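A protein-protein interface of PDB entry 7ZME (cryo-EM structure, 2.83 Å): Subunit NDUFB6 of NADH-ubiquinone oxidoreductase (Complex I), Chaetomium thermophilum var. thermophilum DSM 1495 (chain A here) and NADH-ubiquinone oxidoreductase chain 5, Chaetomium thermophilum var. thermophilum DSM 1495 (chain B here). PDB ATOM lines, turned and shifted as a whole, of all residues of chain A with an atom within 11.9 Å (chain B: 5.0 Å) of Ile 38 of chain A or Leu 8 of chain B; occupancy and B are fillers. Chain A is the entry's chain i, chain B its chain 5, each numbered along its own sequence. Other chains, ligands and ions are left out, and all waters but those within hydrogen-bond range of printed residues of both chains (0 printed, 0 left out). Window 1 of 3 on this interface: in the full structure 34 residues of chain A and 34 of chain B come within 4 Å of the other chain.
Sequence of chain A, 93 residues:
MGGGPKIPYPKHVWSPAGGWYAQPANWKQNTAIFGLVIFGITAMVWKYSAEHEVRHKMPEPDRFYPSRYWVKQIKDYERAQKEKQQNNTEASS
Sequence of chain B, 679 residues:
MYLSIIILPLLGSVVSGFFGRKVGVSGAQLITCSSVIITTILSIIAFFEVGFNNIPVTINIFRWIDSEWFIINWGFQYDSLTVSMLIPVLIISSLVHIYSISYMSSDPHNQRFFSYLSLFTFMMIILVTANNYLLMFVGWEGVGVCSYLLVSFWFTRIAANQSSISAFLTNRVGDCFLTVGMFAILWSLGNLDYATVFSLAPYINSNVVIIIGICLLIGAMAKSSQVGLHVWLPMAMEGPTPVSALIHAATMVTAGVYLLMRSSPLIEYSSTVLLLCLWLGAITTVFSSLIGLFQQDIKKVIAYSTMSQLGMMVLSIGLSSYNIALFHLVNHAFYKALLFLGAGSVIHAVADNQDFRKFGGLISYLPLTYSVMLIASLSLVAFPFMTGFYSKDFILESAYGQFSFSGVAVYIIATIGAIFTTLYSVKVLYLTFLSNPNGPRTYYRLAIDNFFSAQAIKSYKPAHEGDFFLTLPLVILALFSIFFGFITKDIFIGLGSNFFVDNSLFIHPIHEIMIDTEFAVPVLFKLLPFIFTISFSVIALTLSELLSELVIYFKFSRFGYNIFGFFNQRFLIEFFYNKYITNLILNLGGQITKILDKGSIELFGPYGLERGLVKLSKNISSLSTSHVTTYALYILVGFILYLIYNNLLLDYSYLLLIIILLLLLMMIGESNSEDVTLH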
ATOM      1  N   TRP A  27       5.609 -34.950 -26.756  1.00  0.00           N
ATOM      2  CA  TRP A  27       6.895 -34.212 -26.687  1.00  0.00           C
ATOM      3  C   TRP A  27       6.714 -32.707 -26.908  1.00  0.00           C
ATOM      4  O   TRP A  27       7.248 -31.940 -26.125  1.00  0.00           O
ATOM      5  CB  TRP A  27       7.957 -34.861 -27.573  1.00  0.00           C
ATOM      6  CG  TRP A  27       7.912 -34.535 -29.033  1.00  0.00           C
ATOM      7  CD1 TRP A  27       7.371 -35.300 -30.019  1.00  0.00           C
ATOM      8  CD2 TRP A  27       8.483 -33.386 -29.686  1.00  0.00           C
ATOM      9  NE1 TRP A  27       7.543 -34.699 -31.232  1.00  0.00           N
ATOM     10  CE2 TRP A  27       8.218 -33.524 -31.059  1.00  0.00           C
ATOM     11  CE3 TRP A  27       9.160 -32.247 -29.247  1.00  0.00           C
ATOM     12  CZ2 TRP A  27       8.614 -32.571 -31.994  1.00  0.00           C
ATOM     13  CZ3 TRP A  27       9.549 -31.303 -30.168  1.00  0.00           C
ATOM     14  CH2 TRP A  27       9.281 -31.465 -31.524  1.00  0.00           C
ATOM     15  N   LYS A  28       5.949 -32.325 -27.920  1.00  0.00           N
ATOM     16  CA  LYS A  28       5.704 -30.922 -28.236  1.00  0.00           C
ATOM     17  C   LYS A  28       4.971 -30.223 -27.102  1.00  0.00           C
ATOM     18  O   LYS A  28       5.262 -29.065 -26.781  1.00  0.00           O
ATOM     19  CB  LYS A  28       4.906 -30.805 -29.531  1.00  0.00           C
ATOM     20  CG  LYS A  28       5.648 -31.247 -30.771  1.00  0.00           C
ATOM     21  CD  LYS A  28       4.827 -30.978 -32.022  1.00  0.00           C
ATOM     22  CE  LYS A  28       5.397 -31.703 -33.228  1.00  0.00           C
ATOM     23  NZ  LYS A  28       5.322 -33.180 -33.069  1.00  0.00           N
ATOM     24  N   GLN A  29       4.023 -30.873 -26.446  1.00  0.00           N
ATOM     25  CA  GLN A  29       3.180 -30.189 -25.445  1.00  0.00           C
ATOM     26  C   GLN A  29       4.021 -29.911 -24.223  1.00  0.00           C
ATOM     27  O   GLN A  29       3.851 -28.843 -23.629  1.00  0.00           O
ATOM     28  CB  GLN A  29       2.000 -31.095 -25.107  1.00  0.00           C
ATOM     29  CG  GLN A  29       0.952 -30.445 -24.219  1.00  0.00           C
ATOM     30  CD  GLN A  29       0.191 -31.483 -23.431  1.00  0.00           C
ATOM     31  OE1 GLN A  29      -0.875 -31.218 -22.882  1.00  0.00           O
ATOM     32  NE2 GLN A  29       0.744 -32.683 -23.373  1.00  0.00           N
ATOM     33  N   ASN A  30       4.927 -30.829 -23.928  1.00  0.00           N
ATOM     34  CA  ASN A  30       5.775 -30.712 -22.722  1.00  0.00           C
ATOM     35  C   ASN A  30       6.967 -29.812 -23.033  1.00  0.00           C
ATOM     36  O   ASN A  30       7.468 -29.169 -22.100  1.00  0.00           O
ATOM     37  CB  ASN A  30       6.051 -32.114 -22.194  1.00  0.00           C
ATOM     38  CG  ASN A  30       4.730 -32.803 -21.940  1.00  0.00           C
ATOM     39  OD1 ASN A  30       3.988 -33.082 -22.873  1.00  0.00           O
ATOM     40  ND2 ASN A  30       4.381 -33.012 -20.685  1.00  0.00           N
ATOM     41  N   THR A  31       7.365 -29.758 -24.305  1.00  0.00           N
ATOM     42  CA  THR A  31       8.514 -28.907 -24.680  1.00  0.00           C
ATOM     43  C   THR A  31       8.022 -27.481 -24.560  1.00  0.00           C
ATOM     44  O   THR A  31       8.798 -26.629 -24.096  1.00  0.00           O
ATOM     45  CB  THR A  31       9.189 -29.373 -25.974  1.00  0.00           C
ATOM     46  OG1 THR A  31       9.716 -30.677 -25.751  1.00  0.00           O
ATOM     47  CG2 THR A  31      10.294 -28.460 -26.451  1.00  0.00           C
ATOM     48  N   ALA A  32       6.764 -27.252 -24.921  1.00  0.00           N
ATOM     49  CA  ALA A  32       6.153 -25.941 -24.744  1.00  0.00           C
ATOM     50  C   ALA A  32       6.114 -25.550 -23.275  1.00  0.00           C
ATOM     51  O   ALA A  32       6.429 -24.410 -22.919  1.00  0.00           O
ATOM     52  CB  ALA A  32       4.747 -25.936 -25.341  1.00  0.00           C
ATOM     53  N   ILE A  33       5.739 -26.489 -22.404  1.00  0.00           N
ATOM     54  CA  ILE A  33       5.652 -26.197 -20.977  1.00  0.00           C
ATOM     55  C   ILE A  33       7.029 -25.870 -20.413  1.00  0.00           C
ATOM     56  O   ILE A  33       7.197 -24.906 -19.659  1.00  0.00           O
ATOM     57  CB  ILE A  33       5.002 -27.375 -20.231  1.00  0.00           C
ATOM     58  CG1 ILE A  33       3.540 -27.522 -20.640  1.00  0.00           C
ATOM     59  CG2 ILE A  33       5.112 -27.186 -18.731  1.00  0.00           C
ATOM     60  CD1 ILE A  33       2.859 -28.717 -20.022  1.00  0.00           C
ATOM     61  N   PHE A  34       8.035 -26.669 -20.768  1.00  0.00           N
ATOM     62  CA  PHE A  34       9.380 -26.419 -20.264  1.00  0.00           C
ATOM     63  C   PHE A  34       9.978 -25.150 -20.852  1.00  0.00           C
ATOM     64  O   PHE A  34      10.710 -24.436 -20.160  1.00  0.00           O
ATOM     65  CB  PHE A  34      10.283 -27.615 -20.555  1.00  0.00           C
ATOM     66  CG  PHE A  34      10.271 -28.651 -19.477  1.00  0.00           C
ATOM     67  CD1 PHE A  34      10.938 -28.438 -18.291  1.00  0.00           C
ATOM     68  CD2 PHE A  34       9.581 -29.835 -19.646  1.00  0.00           C
ATOM     69  CE1 PHE A  34      10.929 -29.388 -17.300  1.00  0.00           C
ATOM     70  CE2 PHE A  34       9.566 -30.788 -18.657  1.00  0.00           C
ATOM     71  CZ  PHE A  34      10.241 -30.563 -17.485  1.00  0.00           C
ATOM     72  N   GLY A  35       9.688 -24.857 -22.121  1.00  0.00           N
ATOM     73  CA  GLY A  35      10.173 -23.625 -22.716  1.00  0.00           C
ATOM     74  C   GLY A  35       9.615 -22.387 -22.049  1.00  0.00           C
ATOM     75  O   GLY A  35      10.294 -21.361 -21.969  1.00  0.00           O
ATOM     76  N   LEU A  36       8.371 -22.457 -21.575  1.00  0.00           N
ATOM     77  CA  LEU A  36       7.808 -21.356 -20.803  1.00  0.00           C
ATOM     78  C   LEU A  36       8.492 -21.229 -19.449  1.00  0.00           C
ATOM     79  O   LEU A  36       8.721 -20.115 -18.965  1.00  0.00           O
ATOM     80  CB  LEU A  36       6.302 -21.545 -20.631  1.00  0.00           C
ATOM     81  CG  LEU A  36       5.375 -20.925 -21.682  1.00  0.00           C
ATOM     82  CD1 LEU A  36       5.350 -19.412 -21.529  1.00  0.00           C
ATOM     83  CD2 LEU A  36       5.775 -21.307 -23.099  1.00  0.00           C
ATOM     84  N   VAL A  37       8.815 -22.360 -18.820  1.00  0.00           N
ATOM     85  CA  VAL A  37       9.519 -22.327 -17.543  1.00  0.00           C
ATOM     86  C   VAL A  37      10.902 -21.717 -17.716  1.00  0.00           C
ATOM     87  O   VAL A  37      11.346 -20.905 -16.897  1.00  0.00           O
ATOM     88  CB  VAL A  37       9.594 -23.740 -16.938  1.00  0.00           C
ATOM     89  CG1 VAL A  37      10.418 -23.732 -15.660  1.00  0.00           C
ATOM     90  CG2 VAL A  37       8.198 -24.272 -16.667  1.00  0.00           C
ATOM     91  N   ILE A  38      11.604 -22.101 -18.783  1.00  0.00           N
ATOM     92  CA  ILE A  38      12.928 -21.545 -19.044  1.00  0.00           C
ATOM     93  C   ILE A  38      12.838 -20.051 -19.308  1.00  0.00           C
ATOM     94  O   ILE A  38      13.625 -19.265 -18.770  1.00  0.00           O
ATOM     95  CB  ILE A  38      13.599 -22.290 -20.209  1.00  0.00           C
ATOM     96  CG1 ILE A  38      14.137 -23.631 -19.723  1.00  0.00           C
ATOM     97  CG2 ILE A  38      14.704 -21.458 -20.815  1.00  0.00           C
ATOM     98  CD1 ILE A  38      14.387 -24.598 -20.816  1.00  0.00           C
ATOM     99  N   PHE A  39      11.876 -19.636 -20.131  1.00  0.00           N
ATOM    100  CA  PHE A  39      11.689 -18.215 -20.396  1.00  0.00           C
ATOM    101  C   PHE A  39      11.291 -17.471 -19.128  1.00  0.00           C
ATOM    102  O   PHE A  39      11.742 -16.344 -18.892  1.00  0.00           O
ATOM    103  CB  PHE A  39      10.645 -18.029 -21.502  1.00  0.00           C
ATOM    104  CG  PHE A  39      10.239 -16.597 -21.743  1.00  0.00           C
ATOM    105  CD1 PHE A  39       9.275 -15.981 -20.956  1.00  0.00           C
ATOM    106  CD2 PHE A  39      10.781 -15.883 -22.798  1.00  0.00           C
ATOM    107  CE1 PHE A  39       8.899 -14.674 -21.190  1.00  0.00           C
ATOM    108  CE2 PHE A  39      10.408 -14.575 -23.036  1.00  0.00           C
ATOM    109  CZ  PHE A  39       9.463 -13.972 -22.233  1.00  0.00           C
ATOM    110  N   GLY A  40      10.442 -18.084 -18.303  1.00  0.00           N
ATOM    111  CA  GLY A  40       9.921 -17.386 -17.138  1.00  0.00           C
ATOM    112  C   GLY A  40      11.006 -16.982 -16.159  1.00  0.00           C
ATOM    113  O   GLY A  40      11.043 -15.843 -15.688  1.00  0.00           O
ATOM    114  N   ILE A  41      11.909 -17.911 -15.840  1.00  0.00           N
ATOM    115  CA  ILE A  41      12.966 -17.587 -14.891  1.00  0.00           C
ATOM    116  C   ILE A  41      14.141 -16.887 -15.558  1.00  0.00           C
ATOM    117  O   ILE A  41      14.902 -16.193 -14.875  1.00  0.00           O
ATOM    118  CB  ILE A  41      13.427 -18.847 -14.140  1.00  0.00           C
ATOM    119  CG1 ILE A  41      14.013 -19.880 -15.096  1.00  0.00           C
ATOM    120  CG2 ILE A  41      12.271 -19.453 -13.361  1.00  0.00           C
ATOM    121  CD1 ILE A  41      14.683 -21.025 -14.372  1.00  0.00           C
ATOM    122  N   THR A  42      14.316 -17.043 -16.870  1.00  0.00           N
ATOM    123  CA  THR A  42      15.319 -16.252 -17.572  1.00  0.00           C
ATOM    124  C   THR A  42      14.969 -14.773 -17.520  1.00  0.00           C
ATOM    125  O   THR A  42      15.854 -13.918 -17.399  1.00  0.00           O
ATOM    126  CB  THR A  42      15.448 -16.722 -19.021  1.00  0.00           C
ATOM    127  OG1 THR A  42      15.709 -18.130 -19.046  1.00  0.00           O
ATOM    128  CG2 THR A  42      16.585 -15.995 -19.721  1.00  0.00           C
ATOM    129  N   ALA A  43      13.677 -14.456 -17.618  1.00  0.00           N
ATOM    130  CA  ALA A  43      13.232 -13.081 -17.426  1.00  0.00           C
ATOM    131  C   ALA A  43      13.497 -12.613 -16.003  1.00  0.00           C
ATOM    132  O   ALA A  43      13.897 -11.463 -15.784  1.00  0.00           O
ATOM    133  CB  ALA A  43      11.748 -12.961 -17.766  1.00  0.00           C
ATOM    134  N   MET A  44      13.272 -13.487 -15.020  1.00  0.00           N
ATOM    135  CA  MET A  44      13.608 -13.155 -13.641  1.00  0.00           C
ATOM    136  C   MET A  44      15.099 -12.888 -13.491  1.00  0.00           C
ATOM    137  O   MET A  44      15.503 -11.948 -12.800  1.00  0.00           O
ATOM    138  CB  MET A  44      13.171 -14.282 -12.706  1.00  0.00           C
ATOM    139  CG  MET A  44      11.666 -14.462 -12.597  1.00  0.00           C
ATOM    140  SD  MET A  44      11.210 -15.809 -11.488  1.00  0.00           S
ATOM    141  CE  MET A  44       9.427 -15.810 -11.664  1.00  0.00           C
ATOM    142  N   VAL A  45      15.933 -13.715 -14.123  1.00  0.00           N
ATOM    143  CA  VAL A  45      17.368 -13.447 -14.149  1.00  0.00           C
ATOM    144  C   VAL A  45      17.648 -12.135 -14.870  1.00  0.00           C
ATOM    145  O   VAL A  45      18.539 -11.372 -14.481  1.00  0.00           O
ATOM    146  CB  VAL A  45      18.119 -14.626 -14.796  1.00  0.00           C
ATOM    147  CG1 VAL A  45      19.595 -14.313 -14.919  1.00  0.00           C
ATOM    148  CG2 VAL A  45      17.921 -15.881 -13.982  1.00  0.00           C
ATOM    149  N   TRP A  46      16.895 -11.854 -15.935  1.00  0.00           N
ATOM    150  CA  TRP A  46      17.044 -10.581 -16.627  1.00  0.00           C
ATOM    151  C   TRP A  46      16.657  -9.415 -15.729  1.00  0.00           C
ATOM    152  O   TRP A  46      17.344  -8.388 -15.701  1.00  0.00           O
ATOM    153  CB  TRP A  46      16.201 -10.573 -17.901  1.00  0.00           C
ATOM    154  CG  TRP A  46      16.654  -9.571 -18.900  1.00  0.00           C
ATOM    155  CD1 TRP A  46      16.566  -8.215 -18.797  1.00  0.00           C
ATOM    156  CD2 TRP A  46      17.268  -9.838 -20.161  1.00  0.00           C
ATOM    157  NE1 TRP A  46      17.089  -7.620 -19.916  1.00  0.00           N
ATOM    158  CE2 TRP A  46      17.529  -8.595 -20.770  1.00  0.00           C
ATOM    159  CE3 TRP A  46      17.625 -11.007 -20.837  1.00  0.00           C
ATOM    160  CZ2 TRP A  46      18.128  -8.489 -22.017  1.00  0.00           C
ATOM    161  CZ3 TRP A  46      18.219 -10.900 -22.075  1.00  0.00           C
ATOM    162  CH2 TRP A  46      18.465  -9.650 -22.653  1.00  0.00           C
ATOM    163  N   LYS A  47      15.555  -9.552 -14.989  1.00  0.00           N
ATOM    164  CA  LYS A  47      15.143  -8.485 -14.085  1.00  0.00           C
ATOM    165  C   LYS A  47      16.192  -8.235 -13.012  1.00  0.00           C
ATOM    166  O   LYS A  47      16.507  -7.081 -12.698  1.00  0.00           O
ATOM    167  CB  LYS A  47      13.800  -8.822 -13.443  1.00  0.00           C
ATOM    168  CG  LYS A  47      13.274  -7.731 -12.527  1.00  0.00           C
ATOM    169  CD  LYS A  47      11.889  -8.058 -12.000  1.00  0.00           C
ATOM    170  CE  LYS A  47      11.445  -7.032 -10.972  1.00  0.00           C
ATOM    171  NZ  LYS A  47      11.261  -5.689 -11.584  1.00  0.00           N
ATOM    172  N   SER A  49      19.430  -8.937 -13.113  1.00  0.00           N
ATOM    173  CA  SER A  49      20.660  -8.422 -13.703  1.00  0.00           C
ATOM    174  C   SER A  49      20.553  -6.929 -13.981  1.00  0.00           C
ATOM    175  O   SER A  49      21.450  -6.154 -13.633  1.00  0.00           O
ATOM    176  CB  SER A  49      20.974  -9.190 -14.987  1.00  0.00           C
ATOM    177  OG  SER A  49      22.315  -8.992 -15.392  1.00  0.00           O
ATOM    178  N   SER B   4      21.930 -13.479 -17.921  1.00  0.00           N
ATOM    179  CA  SER B   4      21.171 -14.419 -18.733  1.00  0.00           C
ATOM    180  C   SER B   4      22.060 -15.161 -19.719  1.00  0.00           C
ATOM    181  O   SER B   4      21.728 -16.280 -20.121  1.00  0.00           O
ATOM    182  CB  SER B   4      20.059 -13.681 -19.475  1.00  0.00           C
ATOM    183  OG  SER B   4      19.283 -12.909 -18.575  1.00  0.00           O
ATOM    184  N   ILE B   5      23.181 -14.560 -20.118  1.00  0.00           N
ATOM    185  CA  ILE B   5      24.168 -15.283 -20.911  1.00  0.00           C
ATOM    186  C   ILE B   5      24.750 -16.428 -20.096  1.00  0.00           C
ATOM    187  O   ILE B   5      24.995 -17.523 -20.613  1.00  0.00           O
ATOM    188  CB  ILE B   5      25.264 -14.317 -21.400  1.00  0.00           C
ATOM    189  CG1 ILE B   5      24.753 -13.490 -22.573  1.00  0.00           C
ATOM    190  CG2 ILE B   5      26.534 -15.068 -21.784  1.00  0.00           C
ATOM    191  CD1 ILE B   5      25.601 -12.287 -22.879  1.00  0.00           C
ATOM    192  N   ILE B   6      24.968 -16.191 -18.805  1.00  0.00           N
ATOM    193  CA  ILE B   6      25.524 -17.217 -17.933  1.00  0.00           C
ATOM    194  C   ILE B   6      24.511 -18.333 -17.702  1.00  0.00           C
ATOM    195  O   ILE B   6      24.830 -19.518 -17.835  1.00  0.00           O
ATOM    196  CB  ILE B   6      25.978 -16.583 -16.606  1.00  0.00           C
ATOM    197  CG1 ILE B   6      27.159 -15.644 -16.841  1.00  0.00           C
ATOM    198  CG2 ILE B   6      26.317 -17.646 -15.582  1.00  0.00           C
ATOM    199  CD1 ILE B   6      27.274 -14.560 -15.813  1.00  0.00           C
ATOM    200  N   ILE B   7      23.274 -17.972 -17.377  1.00  0.00           N
ATOM    201  CA  ILE B   7      22.352 -18.956 -16.822  1.00  0.00           C
ATOM    202  C   ILE B   7      21.654 -19.767 -17.914  1.00  0.00           C
ATOM    203  O   ILE B   7      21.354 -20.946 -17.709  1.00  0.00           O
ATOM    204  CB  ILE B   7      21.337 -18.253 -15.903  1.00  0.00           C
ATOM    205  CG1 ILE B   7      20.576 -19.270 -15.065  1.00  0.00           C
ATOM    206  CG2 ILE B   7      20.354 -17.430 -16.716  1.00  0.00           C
ATOM    207  CD1 ILE B   7      21.448 -20.002 -14.078  1.00  0.00           C
ATOM    208  N   LEU B   8      21.409 -19.175 -19.083  1.00  0.00           N
ATOM    209  CA  LEU B   8      20.538 -19.812 -20.069  1.00  0.00           C
ATOM    210  C   LEU B   8      21.027 -21.177 -20.547  1.00  0.00           C
ATOM    211  O   LEU B   8      20.195 -22.098 -20.629  1.00  0.00           O
ATOM    212  CB  LEU B   8      20.326 -18.862 -21.256  1.00  0.00           C
ATOM    213  CG  LEU B   8      19.174 -19.193 -22.200  1.00  0.00           C
ATOM    214  CD1 LEU B   8      17.967 -19.695 -21.427  1.00  0.00           C
ATOM    215  CD2 LEU B   8      18.808 -17.980 -23.025  1.00  0.00           C
ATOM    216  N   PRO B   9      22.305 -21.385 -20.887  1.00  0.00           N
ATOM    217  CA  PRO B   9      22.748 -22.744 -21.245  1.00  0.00           C
ATOM    218  C   PRO B   9      22.579 -23.758 -20.125  1.00  0.00           C
ATOM    219  O   PRO B   9      22.406 -24.947 -20.418  1.00  0.00           O
ATOM    220  CB  PRO B   9      24.225 -22.549 -21.605  1.00  0.00           C
ATOM    221  CG  PRO B   9      24.336 -21.117 -21.958  1.00  0.00           C
ATOM    222  CD  PRO B   9      23.408 -20.420 -21.030  1.00  0.00           C
ATOM    223  N   LEU B  10      22.622 -23.330 -18.862  1.00  0.00           N
ATOM    224  CA  LEU B  10      22.408 -24.244 -17.747  1.00  0.00           C
ATOM    225  C   LEU B  10      20.985 -24.792 -17.714  1.00  0.00           C
ATOM    226  O   LEU B  10      20.790 -25.968 -17.396  1.00  0.00           O
ATOM    227  CB  LEU B  10      22.747 -23.544 -16.432  1.00  0.00           C
ATOM    228  CG  LEU B  10      22.445 -24.270 -15.122  1.00  0.00           C
ATOM    229  CD1 LEU B  10      23.190 -25.584 -15.049  1.00  0.00           C
ATOM    230  CD2 LEU B  10      22.822 -23.399 -13.948  1.00  0.00           C
ATOM    231  N   LEU B  11      19.989 -23.966 -18.037  1.00  0.00           N
ATOM    232  CA  LEU B  11      18.602 -24.423 -18.064  1.00  0.00           C
ATOM    233  C   LEU B  11      18.341 -25.453 -19.150  1.00  0.00           C
ATOM    234  O   LEU B  11      17.591 -26.406 -18.919  1.00  0.00           O
ATOM    235  CB  LEU B  11      17.654 -23.241 -18.258  1.00  0.00           C
ATOM    236  CG  LEU B  11      17.328 -22.338 -17.079  1.00  0.00           C
ATOM    237  CD1 LEU B  11      18.491 -21.493 -16.700  1.00  0.00           C
ATOM    238  CD2 LEU B  11      16.189 -21.453 -17.491  1.00  0.00           C
ATOM    239  N   GLY B  12      18.920 -25.270 -20.336  1.00  0.00           N
ATOM    240  CA  GLY B  12      18.751 -26.260 -21.383  1.00  0.00           C
ATOM    241  C   GLY B  12      19.272 -27.626 -20.982  1.00  0.00           C
ATOM    242  O   GLY B  12      18.624 -28.644 -21.229  1.00  0.00           O
ATOM    243  N   VAL B  15      16.941 -29.436 -18.281  1.00  0.00           N
ATOM    244  CA  VAL B  15      15.722 -30.005 -18.843  1.00  0.00           C
ATOM    245  C   VAL B  15      16.055 -31.181 -19.750  1.00  0.00           C
ATOM    246  O   VAL B  15      15.398 -32.227 -19.699  1.00  0.00           O
ATOM    247  CB  VAL B  15      14.919 -28.919 -19.581  1.00  0.00           C
ATOM    248  CG1 VAL B  15      13.766 -29.534 -20.347  1.00  0.00           C
ATOM    249  CG2 VAL B  15      14.414 -27.890 -18.601  1.00  0.00           C
ATOM    250  N   ILE B  31      15.284 -27.380 -27.208  1.00  0.00           N
ATOM    251  CA  ILE B  31      15.528 -26.548 -26.037  1.00  0.00           C
ATOM    252  C   ILE B  31      17.007 -26.210 -25.904  1.00  0.00           C
ATOM    253  O   ILE B  31      17.376 -25.043 -25.730  1.00  0.00           O
ATOM    254  CB  ILE B  31      14.990 -27.245 -24.776  1.00  0.00           C
ATOM    255  CG1 ILE B  31      13.470 -27.364 -24.853  1.00  0.00           C
ATOM    256  CG2 ILE B  31      15.439 -26.512 -23.528  1.00  0.00           C
ATOM    257  CD1 ILE B  31      12.805 -27.670 -23.528  1.00  0.00           C
ATOM    258  N   SER B  35      18.597 -22.449 -26.470  1.00  0.00           N
ATOM    259  CA  SER B  35      19.262 -21.783 -25.358  1.00  0.00           C
ATOM    260  C   SER B  35      20.671 -21.348 -25.728  1.00  0.00           C
ATOM    261  O   SER B  35      21.204 -20.404 -25.135  1.00  0.00           O
ATOM    262  CB  SER B  35      19.294 -22.703 -24.138  1.00  0.00           C
ATOM    263  OG  SER B  35      17.985 -23.040 -23.715  1.00  0.00           O
ATOM    264  N   ILE B  38      20.216 -18.345 -28.594  1.00  0.00           N
ATOM    265  CA  ILE B  38      19.830 -17.106 -27.926  1.00  0.00           C
ATOM    266  C   ILE B  38      20.991 -16.556 -27.108  1.00  0.00           C
ATOM    267  O   ILE B  38      21.253 -15.348 -27.114  1.00  0.00           O
ATOM    268  CB  ILE B  38      18.578 -17.340 -27.059  1.00  0.00           C
ATOM    269  CG1 ILE B  38      17.354 -17.529 -27.946  1.00  0.00           C
ATOM    270  CG2 ILE B  38      18.342 -16.171 -26.132  1.00  0.00           C
ATOM    271  CD1 ILE B  38      16.110 -17.903 -27.182  1.00  0.00           C
ATOM    272  N   THR B  39      21.706 -17.430 -26.397  1.00  0.00           N
ATOM    273  CA  THR B  39      22.889 -16.999 -25.655  1.00  0.00           C
ATOM    274  C   THR B  39      23.964 -16.474 -26.596  1.00  0.00           C
ATOM    275  O   THR B  39      24.689 -15.532 -26.257  1.00  0.00           O
ATOM    276  CB  THR B  39      23.428 -18.154 -24.813  1.00  0.00           C
ATOM    277  OG1 THR B  39      22.355 -18.736 -24.064  1.00  0.00           O
ATOM    278  CG2 THR B  39      24.497 -17.669 -23.857  1.00  0.00           C
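Val 15 of chain B touches Phe 34 of chain A. Phe 34 of chain A touches Ile 31 of chain B (CB to CD1, 3.9 Å). Ile 38 of chain A touches Leu 8 of chain B. Leu 11 of chain B touches Ile 38 of chain A. Val 15 of chain B touches Ile 38 of chain A. Leu 11 of chain B touches Ile 41 of chain A. Leu 11 of chain B touches Thr 42 of chain A. Val 45 of chain A touches Ser 4 of chain B (CG1 to N, 3.9 Å). Val 45 of chain A touches Ile 7 of chain B (CG1 to CG2, 3.7 Å). Trp 46 of chain A touches Ser 4 of chain B (CE3 to OG, 3.4 Å).
Printed residues of chain B that touch a printed residue of chain A: Ser 4, Ile 7, Leu 8, Leu 11, Val 15 and Ile 31. Hydrophobic or aromatic side chains of chain B that line the printed part of chain A: Ile 7, Leu 8, Leu 11, Val 15 and Ile 31. Of the 22 printed residues of chain A, 7 touch a printed residue of chain B. Hydrophobic or aromatic side chains of chain A that line the printed part of chain B: Phe 34, Ile 38, Ile 41, Val 45 and Trp 46. Among the printed residues, 14 pairs touch across the chains.
The backbone carbonyl oxygen (O) of Trp 27 of chain A lies within hydrogen-bond range of the side-chain hydroxyl (OG1) of Thr 31 of chain A, 2.8 Å away. The side-chain hydroxyl (OG) of Ser 35 of chain B lies within hydrogen-bond range of the backbone carbonyl oxygen (O) of Ile 31 of chain B (2.9 Å).
Of the printed residues of chain A, Leu 8 of chain B touches Ile 38 and Thr 42. Of chain A, only Thr 42, Val 45 and Trp 46 come within 4 Å of Ser 4 of chain B. Of the printed residues of chain A, Ile 7 of chain B touches Val 45 (3.7 Å). Leu 11 of chain B touches just these residues of chain A: Ile 38, Ile 41 and Thr 42. Of chain A, only Phe 34 and Ile 38 come within 4 Å of Val 15 of chain B. Ile 31 of chain B touches three residues of chain A. No residue of chain A comes within 4 Å of Ser 35 of chain B. No residue of chain A comes within 4 Å of Thr 39 of chain B. Of the printed residues of chain B, Phe 34 of chain A touches Val 15 (3.5 Å) and Ile 31 (3.9 Å). Of the printed residues of chain B, Val 45 of chain A touches Ser 4 (3.9 Å) and Ile 7 (3.7 Å). Of the printed residues of chain B, Thr 31 of chain A touches Ile 31. Of the printed residues of chain B, Trp 46 of chain A touches Ser 4. Printed residues of chain B within 4 Å of Ile 41 of chain A: Leu 11. The nearest residue of chain B that does not touch Ile 38 of chain A is Gly 12 of chain B (4.6 Å). The nearest residue of chain A that does not touch Leu 8 of chain B is Phe 39 of chain A (6.2 Å). The nearest printed residue of chain B that does not touch Ile 41 of chain A is Ile 7 of chain B (5.9 Å).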
